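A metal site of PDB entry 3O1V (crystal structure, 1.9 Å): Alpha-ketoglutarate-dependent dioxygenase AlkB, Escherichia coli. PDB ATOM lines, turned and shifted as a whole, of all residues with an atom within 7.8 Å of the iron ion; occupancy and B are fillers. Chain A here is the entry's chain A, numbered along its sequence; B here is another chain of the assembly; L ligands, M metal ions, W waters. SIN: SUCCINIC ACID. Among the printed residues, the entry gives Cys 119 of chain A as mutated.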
ATOM      1  N   LEU A 108      11.101   3.222 -25.222  1.00  0.00           N
ATOM      2  CA  LEU A 108      10.305   4.409 -25.430  1.00  0.00           C
ATOM      3  C   LEU A 108      10.747   5.463 -24.447  1.00  0.00           C
ATOM      4  O   LEU A 108      10.885   5.188 -23.247  1.00  0.00           O
ATOM      5  CB  LEU A 108       8.802   4.099 -25.246  1.00  0.00           C
ATOM      6  CG  LEU A 108       7.768   5.205 -25.205  1.00  0.00           C
ATOM      7  CD1 LEU A 108       7.696   5.979 -26.526  1.00  0.00           C
ATOM      8  CD2 LEU A 108       6.354   4.629 -24.845  1.00  0.00           C
ATOM      9  N   ASN A 110       9.826   9.032 -22.763  1.00  0.00           N
ATOM     10  CA  ASN A 110       8.767  10.027 -22.499  1.00  0.00           C
ATOM     11  C   ASN A 110       9.386  11.256 -21.849  1.00  0.00           C
ATOM     12  O   ASN A 110      10.263  11.122 -20.951  1.00  0.00           O
ATOM     13  CB  ASN A 110       7.740   9.485 -21.478  1.00  0.00           C
ATOM     14  CG  ASN A 110       6.858   8.366 -22.033  1.00  0.00           C
ATOM     15  OD1 ASN A 110       6.087   7.726 -21.291  1.00  0.00           O
ATOM     16  ND2 ASN A 110       6.915   8.182 -23.324  1.00  0.00           N
ATOM     17  N   LEU A 118      -0.116  10.702 -17.696  1.00  0.00           N
ATOM     18  CA  LEU A 118      -0.358   9.492 -18.467  1.00  0.00           C
ATOM     19  C   LEU A 118      -1.381   8.704 -17.730  1.00  0.00           C
ATOM     20  O   LEU A 118      -1.069   8.159 -16.654  1.00  0.00           O
ATOM     21  CB  LEU A 118       0.902   8.651 -18.583  1.00  0.00           C
ATOM     22  CG  LEU A 118       1.070   7.711 -19.776  1.00  0.00           C
ATOM     23  CD1 LEU A 118       1.054   8.543 -21.099  1.00  0.00           C
ATOM     24  CD2 LEU A 118       2.379   6.881 -19.671  1.00  0.00           C
ATOM     25  N   CYS A 119      -2.577   8.608 -18.337  1.00  0.00           N
ATOM     26  CA  CYS A 119      -3.725   7.937 -17.736  1.00  0.00           C
ATOM     27  C   CYS A 119      -3.547   6.432 -17.627  1.00  0.00           C
ATOM     28  O   CYS A 119      -2.797   5.809 -18.402  1.00  0.00           O
ATOM     29  CB  CYS A 119      -5.013   8.239 -18.567  1.00  0.00           C
ATOM     30  SG  CYS A 119      -5.691   9.956 -18.381  1.00  0.00           S
ATOM     31  N   LEU A 120      -4.233   5.826 -16.660  1.00  0.00           N
ATOM     32  CA  LEU A 120      -3.990   4.393 -16.390  1.00  0.00           C
ATOM     33  C   LEU A 120      -4.090   3.556 -17.630  1.00  0.00           C
ATOM     34  O   LEU A 120      -5.062   3.623 -18.369  1.00  0.00           O
ATOM     35  CB  LEU A 120      -5.024   3.820 -15.410  1.00  0.00           C
ATOM     36  CG  LEU A 120      -5.035   4.189 -13.956  1.00  0.00           C
ATOM     37  CD1 LEU A 120      -6.199   3.373 -13.271  1.00  0.00           C
ATOM     38  CD2 LEU A 120      -3.639   3.796 -13.328  1.00  0.00           C
ATOM     39  N   HIS A 121      -3.099   2.730 -17.861  1.00  0.00           N
ATOM     40  CA  HIS A 121      -3.154   1.870 -19.022  1.00  0.00           C
ATOM     41  C   HIS A 121      -2.370   0.616 -18.722  1.00  0.00           C
ATOM     42  O   HIS A 121      -1.677   0.513 -17.663  1.00  0.00           O
ATOM     43  CB  HIS A 121      -2.517   2.586 -20.194  1.00  0.00           C
ATOM     44  CG  HIS A 121      -1.056   2.849 -19.977  1.00  0.00           C
ATOM     45  ND1 HIS A 121      -0.587   3.921 -19.254  1.00  0.00           N
ATOM     46  CD2 HIS A 121       0.037   2.120 -20.328  1.00  0.00           C
ATOM     47  CE1 HIS A 121       0.737   3.876 -19.189  1.00  0.00           C
ATOM     48  NE2 HIS A 121       1.134   2.768 -19.810  1.00  0.00           N
ATOM     49  N   GLN A 122      -2.415  -0.333 -19.655  1.00  0.00           N
ATOM     50  CA  GLN A 122      -1.632  -1.580 -19.528  1.00  0.00           C
ATOM     51  C   GLN A 122      -0.625  -1.567 -20.663  1.00  0.00           C
ATOM     52  O   GLN A 122      -0.981  -1.144 -21.751  1.00  0.00           O
ATOM     53  CB  GLN A 122      -2.522  -2.778 -19.797  1.00  0.00           C
ATOM     54  CG  GLN A 122      -3.474  -3.026 -18.726  1.00  0.00           C
ATOM     55  CD  GLN A 122      -4.434  -4.151 -19.060  1.00  0.00           C
ATOM     56  OE1 GLN A 122      -5.267  -4.017 -19.971  1.00  0.00           O
ATOM     57  NE2 GLN A 122      -4.317  -5.270 -18.347  1.00  0.00           N
ATOM     58  N   ASP A 123       0.609  -2.054 -20.432  1.00  0.00           N
ATOM     59  CA  ASP A 123       1.508  -2.298 -21.553  1.00  0.00           C
ATOM     60  C   ASP A 123       1.258  -3.675 -22.106  1.00  0.00           C
ATOM     61  O   ASP A 123       1.632  -4.650 -21.499  1.00  0.00           O
ATOM     62  CB  ASP A 123       2.948  -2.148 -21.142  1.00  0.00           C
ATOM     63  CG  ASP A 123       3.322  -0.715 -21.017  1.00  0.00           C
ATOM     64  OD1 ASP A 123       2.909  -0.124 -20.054  1.00  0.00           O
ATOM     65  OD2 ASP A 123       3.979  -0.143 -21.927  1.00  0.00           O
ATOM     66  N   LYS A 124       0.586  -3.773 -23.246  1.00  0.00           N
ATOM     67  CA  LYS A 124       0.273  -5.110 -23.639  1.00  0.00           C
ATOM     68  C   LYS A 124       0.535  -5.409 -25.105  1.00  0.00           C
ATOM     69  O   LYS A 124       0.060  -6.415 -25.629  1.00  0.00           O
ATOM     70  CB  LYS A 124      -1.136  -5.496 -23.173  1.00  0.00           C
ATOM     71  CG  LYS A 124      -2.298  -4.720 -23.779  1.00  0.00           C
ATOM     72  CD  LYS A 124      -3.584  -5.317 -23.184  1.00  0.00           C
ATOM     73  CE  LYS A 124      -4.864  -4.638 -23.663  1.00  0.00           C
ATOM     74  NZ  LYS A 124      -4.860  -4.491 -25.138  1.00  0.00           N
ATOM     75  N   GLU A 126       3.454  -6.090 -26.478  1.00  0.00           N
ATOM     76  CA  GLU A 126       4.600  -6.943 -26.643  1.00  0.00           C
ATOM     77  C   GLU A 126       4.116  -8.394 -26.795  1.00  0.00           C
ATOM     78  O   GLU A 126       3.337  -8.882 -25.990  1.00  0.00           O
ATOM     79  CB  GLU A 126       5.478  -6.814 -25.410  1.00  0.00           C
ATOM     80  CG  GLU A 126       5.981  -5.379 -25.152  1.00  0.00           C
ATOM     81  CD  GLU A 126       4.928  -4.393 -24.613  1.00  0.00           C
ATOM     82  OE1 GLU A 126       5.059  -3.170 -24.894  1.00  0.00           O
ATOM     83  OE2 GLU A 126       3.983  -4.827 -23.908  1.00  0.00           O
ATOM     84  N   ILE A 133       8.880  -5.244 -17.923  1.00  0.00           N
ATOM     85  CA  ILE A 133       9.103  -3.869 -18.357  1.00  0.00           C
ATOM     86  C   ILE A 133      10.098  -3.246 -17.379  1.00  0.00           C
ATOM     87  O   ILE A 133       9.941  -3.386 -16.151  1.00  0.00           O
ATOM     88  CB  ILE A 133       7.812  -3.066 -18.265  1.00  0.00           C
ATOM     89  CG1 ILE A 133       6.728  -3.687 -19.137  1.00  0.00           C
ATOM     90  CG2 ILE A 133       8.048  -1.537 -18.592  1.00  0.00           C
ATOM     91  CD1 ILE A 133       6.972  -3.570 -20.633  1.00  0.00           C
ATOM     92  N   SER A 135      11.510   0.472 -16.193  1.00  0.00           N
ATOM     93  CA  SER A 135      11.156   1.918 -16.268  1.00  0.00           C
ATOM     94  C   SER A 135      12.126   2.761 -15.444  1.00  0.00           C
ATOM     95  O   SER A 135      12.192   2.605 -14.221  1.00  0.00           O
ATOM     96  CB  SER A 135       9.694   2.088 -15.813  1.00  0.00           C
ATOM     97  OG  SER A 135       9.257   3.483 -15.717  1.00  0.00           O
ATOM     98  N   PHE A 144       3.587   8.040  -9.381  1.00  0.00           N
ATOM     99  CA  PHE A 144       3.302   6.821 -10.190  1.00  0.00           C
ATOM    100  C   PHE A 144       2.126   6.102  -9.541  1.00  0.00           C
ATOM    101  O   PHE A 144       2.151   5.860  -8.311  1.00  0.00           O
ATOM    102  CB  PHE A 144       4.561   5.965 -10.163  1.00  0.00           C
ATOM    103  CG  PHE A 144       4.504   4.659 -10.992  1.00  0.00           C
ATOM    104  CD1 PHE A 144       4.398   4.692 -12.390  1.00  0.00           C
ATOM    105  CD2 PHE A 144       4.654   3.437 -10.371  1.00  0.00           C
ATOM    106  CE1 PHE A 144       4.376   3.497 -13.146  1.00  0.00           C
ATOM    107  CE2 PHE A 144       4.671   2.221 -11.141  1.00  0.00           C
ATOM    108  CZ  PHE A 144       4.499   2.274 -12.530  1.00  0.00           C
ATOM    109  N   TRP A 168       8.344  -4.229 -13.579  1.00  0.00           N
ATOM    110  CA  TRP A 168       7.260  -5.163 -13.363  1.00  0.00           C
ATOM    111  C   TRP A 168       7.263  -6.341 -14.370  1.00  0.00           C
ATOM    112  O   TRP A 168       7.755  -6.236 -15.490  1.00  0.00           O
ATOM    113  CB  TRP A 168       5.896  -4.501 -13.227  1.00  0.00           C
ATOM    114  CG  TRP A 168       5.431  -3.667 -14.390  1.00  0.00           C
ATOM    115  CD1 TRP A 168       4.482  -4.011 -15.322  1.00  0.00           C
ATOM    116  CD2 TRP A 168       5.825  -2.317 -14.685  1.00  0.00           C
ATOM    117  NE1 TRP A 168       4.287  -2.952 -16.207  1.00  0.00           N
ATOM    118  CE2 TRP A 168       5.099  -1.913 -15.823  1.00  0.00           C
ATOM    119  CE3 TRP A 168       6.731  -1.430 -14.096  1.00  0.00           C
ATOM    120  CZ2 TRP A 168       5.269  -0.667 -16.393  1.00  0.00           C
ATOM    121  CZ3 TRP A 168       6.888  -0.155 -14.679  1.00  0.00           C
ATOM    122  CH2 TRP A 168       6.170   0.199 -15.814  1.00  0.00           C
ATOM    123  N   PHE A 175      -0.498  -5.324 -15.127  1.00  0.00           N
ATOM    124  CA  PHE A 175      -1.133  -4.401 -14.193  1.00  0.00           C
ATOM    125  C   PHE A 175      -1.245  -2.986 -14.785  1.00  0.00           C
ATOM    126  O   PHE A 175      -0.371  -2.517 -15.462  1.00  0.00           O
ATOM    127  CB  PHE A 175      -0.395  -4.347 -12.827  1.00  0.00           C
ATOM    128  CG  PHE A 175      -0.646  -5.568 -11.937  1.00  0.00           C
ATOM    129  CD1 PHE A 175      -0.161  -5.602 -10.630  1.00  0.00           C
ATOM    130  CD2 PHE A 175      -1.341  -6.664 -12.412  1.00  0.00           C
ATOM    131  CE1 PHE A 175      -0.374  -6.703  -9.779  1.00  0.00           C
ATOM    132  CE2 PHE A 175      -1.590  -7.786 -11.556  1.00  0.00           C
ATOM    133  CZ  PHE A 175      -1.094  -7.792 -10.238  1.00  0.00           C
ATOM    134  N   TYR A 176      -2.343  -2.330 -14.473  1.00  0.00           N
ATOM    135  CA  TYR A 176      -2.568  -0.939 -14.890  1.00  0.00           C
ATOM    136  C   TYR A 176      -1.666  -0.001 -14.111  1.00  0.00           C
ATOM    137  O   TYR A 176      -1.452  -0.182 -12.913  1.00  0.00           O
ATOM    138  CB  TYR A 176      -3.998  -0.515 -14.653  1.00  0.00           C
ATOM    139  CG  TYR A 176      -4.997  -0.978 -15.689  1.00  0.00           C
ATOM    140  CD1 TYR A 176      -5.355  -0.172 -16.753  1.00  0.00           C
ATOM    141  CD2 TYR A 176      -5.627  -2.201 -15.560  1.00  0.00           C
ATOM    142  CE1 TYR A 176      -6.258  -0.572 -17.686  1.00  0.00           C
ATOM    143  CE2 TYR A 176      -6.559  -2.615 -16.486  1.00  0.00           C
ATOM    144  CZ  TYR A 176      -6.870  -1.800 -17.533  1.00  0.00           C
ATOM    145  OH  TYR A 176      -7.812  -2.235 -18.440  1.00  0.00           O
ATOM    146  N   HIS A 177      -1.184   1.023 -14.794  1.00  0.00           N
ATOM    147  CA  HIS A 177      -0.336   2.002 -14.178  1.00  0.00           C
ATOM    148  C   HIS A 177      -0.383   3.297 -14.968  1.00  0.00           C
ATOM    149  O   HIS A 177      -0.848   3.380 -16.142  1.00  0.00           O
ATOM    150  CB  HIS A 177       1.117   1.434 -14.172  1.00  0.00           C
ATOM    151  CG  HIS A 177       1.614   1.096 -15.538  1.00  0.00           C
ATOM    152  ND1 HIS A 177       1.434  -0.152 -16.105  1.00  0.00           N
ATOM    153  CD2 HIS A 177       2.235   1.843 -16.481  1.00  0.00           C
ATOM    154  CE1 HIS A 177       1.905  -0.151 -17.336  1.00  0.00           C
ATOM    155  NE2 HIS A 177       2.413   1.034 -17.585  1.00  0.00           N
ATOM    156  N   GLY A 178       0.131   4.352 -14.338  1.00  0.00           N
ATOM    157  CA  GLY A 178       0.103   5.676 -14.944  1.00  0.00           C
ATOM    158  C   GLY A 178       0.797   6.737 -14.143  1.00  0.00           C
ATOM    159  O   GLY A 178       1.434   6.426 -13.094  1.00  0.00           O
ATOM    160  N   ASN A 196      11.320   9.743 -18.715  1.00  0.00           N
ATOM    161  CA  ASN A 196      11.197   8.326 -18.354  1.00  0.00           C
ATOM    162  C   ASN A 196      11.635   7.444 -19.505  1.00  0.00           C
ATOM    163  O   ASN A 196      11.235   7.699 -20.675  1.00  0.00           O
ATOM    164  CB  ASN A 196       9.753   7.978 -17.947  1.00  0.00           C
ATOM    165  CG  ASN A 196       9.597   6.500 -17.639  1.00  0.00           C
ATOM    166  OD1 ASN A 196       9.020   5.769 -18.433  1.00  0.00           O
ATOM    167  ND2 ASN A 196      10.181   6.056 -16.542  1.00  0.00           N
ATOM    168  N   THR A 198      11.280   3.659 -20.789  1.00  0.00           N
ATOM    169  CA  THR A 198      10.694   2.311 -20.638  1.00  0.00           C
ATOM    170  C   THR A 198      11.276   1.297 -21.669  1.00  0.00           C
ATOM    171  O   THR A 198      10.977   1.369 -22.896  1.00  0.00           O
ATOM    172  CB  THR A 198       9.139   2.342 -20.730  1.00  0.00           C
ATOM    173  OG1 THR A 198       8.612   3.223 -19.706  1.00  0.00           O
ATOM    174  CG2 THR A 198       8.551   0.947 -20.516  1.00  0.00           C
ATOM    175  N   ARG A 200      11.538  -2.515 -23.308  1.00  0.00           N
ATOM    176  CA  ARG A 200      10.647  -3.628 -23.581  1.00  0.00           C
ATOM    177  C   ARG A 200      11.284  -4.547 -24.576  1.00  0.00           C
ATOM    178  O   ARG A 200      12.122  -4.108 -25.420  1.00  0.00           O
ATOM    179  CB  ARG A 200       9.313  -3.141 -24.213  1.00  0.00           C
ATOM    180  CG  ARG A 200       8.591  -1.919 -23.518  1.00  0.00           C
ATOM    181  CD  ARG A 200       8.728  -0.600 -24.339  1.00  0.00           C
ATOM    182  NE  ARG A 200       8.079   0.511 -23.628  1.00  0.00           N
ATOM    183  CZ  ARG A 200       6.782   0.782 -23.728  1.00  0.00           C
ATOM    184  NH1 ARG A 200       6.019   0.046 -24.523  1.00  0.00           N
ATOM    185  NH2 ARG A 200       6.249   1.789 -23.044  1.00  0.00           N
ATOM    186  P   MDJ B   7      -5.423   3.395 -22.921  1.00  0.00           P
ATOM    187  N1  MDJ B   7      -0.624   4.719 -23.551  1.00  0.00           N
ATOM    188  C2  MDJ B   7       0.798   4.552 -23.576  1.00  0.00           C
ATOM    189  O2  MDJ B   7       1.654   5.514 -23.496  1.00  0.00           O
ATOM    190  C3  MDJ B   7       1.356   3.324 -23.832  1.00  0.00           C
ATOM    191  C4  MDJ B   7       0.553   2.220 -23.949  1.00  0.00           C
ATOM    192  N4  MDJ B   7       1.104   1.008 -24.165  1.00  0.00           N
ATOM    193  C5  MDJ B   7      -0.834   2.362 -23.866  1.00  0.00           C
ATOM    194  C6  MDJ B   7      -1.435   3.589 -23.607  1.00  0.00           C
ATOM    195  C1' MDJ B   7      -1.349   5.954 -23.191  1.00  0.00           C
ATOM    196  O1P MDJ B   7      -4.882   2.628 -24.110  1.00  0.00           O
ATOM    197  C2' MDJ B   7      -2.585   6.283 -24.085  1.00  0.00           C
ATOM    198  C20 MDJ B   7       2.868   3.313 -23.920  1.00  0.00           C
ATOM    199  O21 MDJ B   7       3.594   2.119 -24.159  1.00  0.00           O
ATOM    200  O2P MDJ B   7      -5.355   2.706 -21.594  1.00  0.00           O
ATOM    201  C3' MDJ B   7      -3.424   7.179 -23.163  1.00  0.00           C
ATOM    202  O3' MDJ B   7      -2.637   8.470 -23.127  1.00  0.00           O
ATOM    203  C4' MDJ B   7      -3.329   6.482 -21.872  1.00  0.00           C
ATOM    204  O4' MDJ B   7      -2.108   5.647 -21.974  1.00  0.00           O
ATOM    205  C5' MDJ B   7      -4.590   5.568 -21.716  1.00  0.00           C
ATOM    206  O5' MDJ B   7      -4.502   4.787 -22.938  1.00  0.00           O
HETATM  207  C1  SIN L   1       4.777   3.933 -18.209  1.00  0.00           C
HETATM  208  O1  SIN L   1       3.552   3.870 -18.376  1.00  0.00           O
HETATM  209  O2  SIN L   1       5.405   2.849 -18.134  1.00  0.00           O
HETATM  210  C2  SIN L   1       5.471   5.246 -18.088  1.00  0.00           C
HETATM  211  C3  SIN L   1       5.443   5.644 -16.628  1.00  0.00           C
HETATM  212  C4  SIN L   1       6.513   6.718 -16.385  1.00  0.00           C
HETATM  213  O3  SIN L   1       6.665   7.701 -17.140  1.00  0.00           O
HETATM  214  O4  SIN L   1       7.264   6.663 -15.389  1.00  0.00           O
HETATM  215 FE    FE M   1       3.177   1.923 -19.403  1.00  0.00          FE
HETATM  216  O   HOH W   1       4.261   2.173 -20.980  1.00  0.00           O
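A ring nitrogen (ND1) of His 177 sits at hydrogen-bond distance from the backbone carbonyl oxygen (O) of Phe 175 (3.0 Å).
OD2 of Asp 123 is in salt-bridge range of NH2 of Arg 200, at 3.2 Å.
ND1 of His 121 sits at hydrogen-bond distance from O of Cys 119 (3.0 Å).
Of the 22 residues printed, 3 come within 4 Å of the iron ion.
The iron ion is bound by water W1 (1.9 Å), NE2 of His 177 (2.2 Å), OD1 of Asp 123 (2.2 Å), O1 of the ligand (2.2 Å) and NE2 of His 121 (2.2 Å).
The iron ion has five donor atoms within binding distance.
Slightly farther from the iron ion lies O2 of the ligand (2.7 Å).
Water W1 lies within hydrogen-bond range of the side-chain carboxylate (OD2) of Asp 123, the guanidinium group (NH2) of Arg 200 and O21 of MDJ 7 of chain B.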
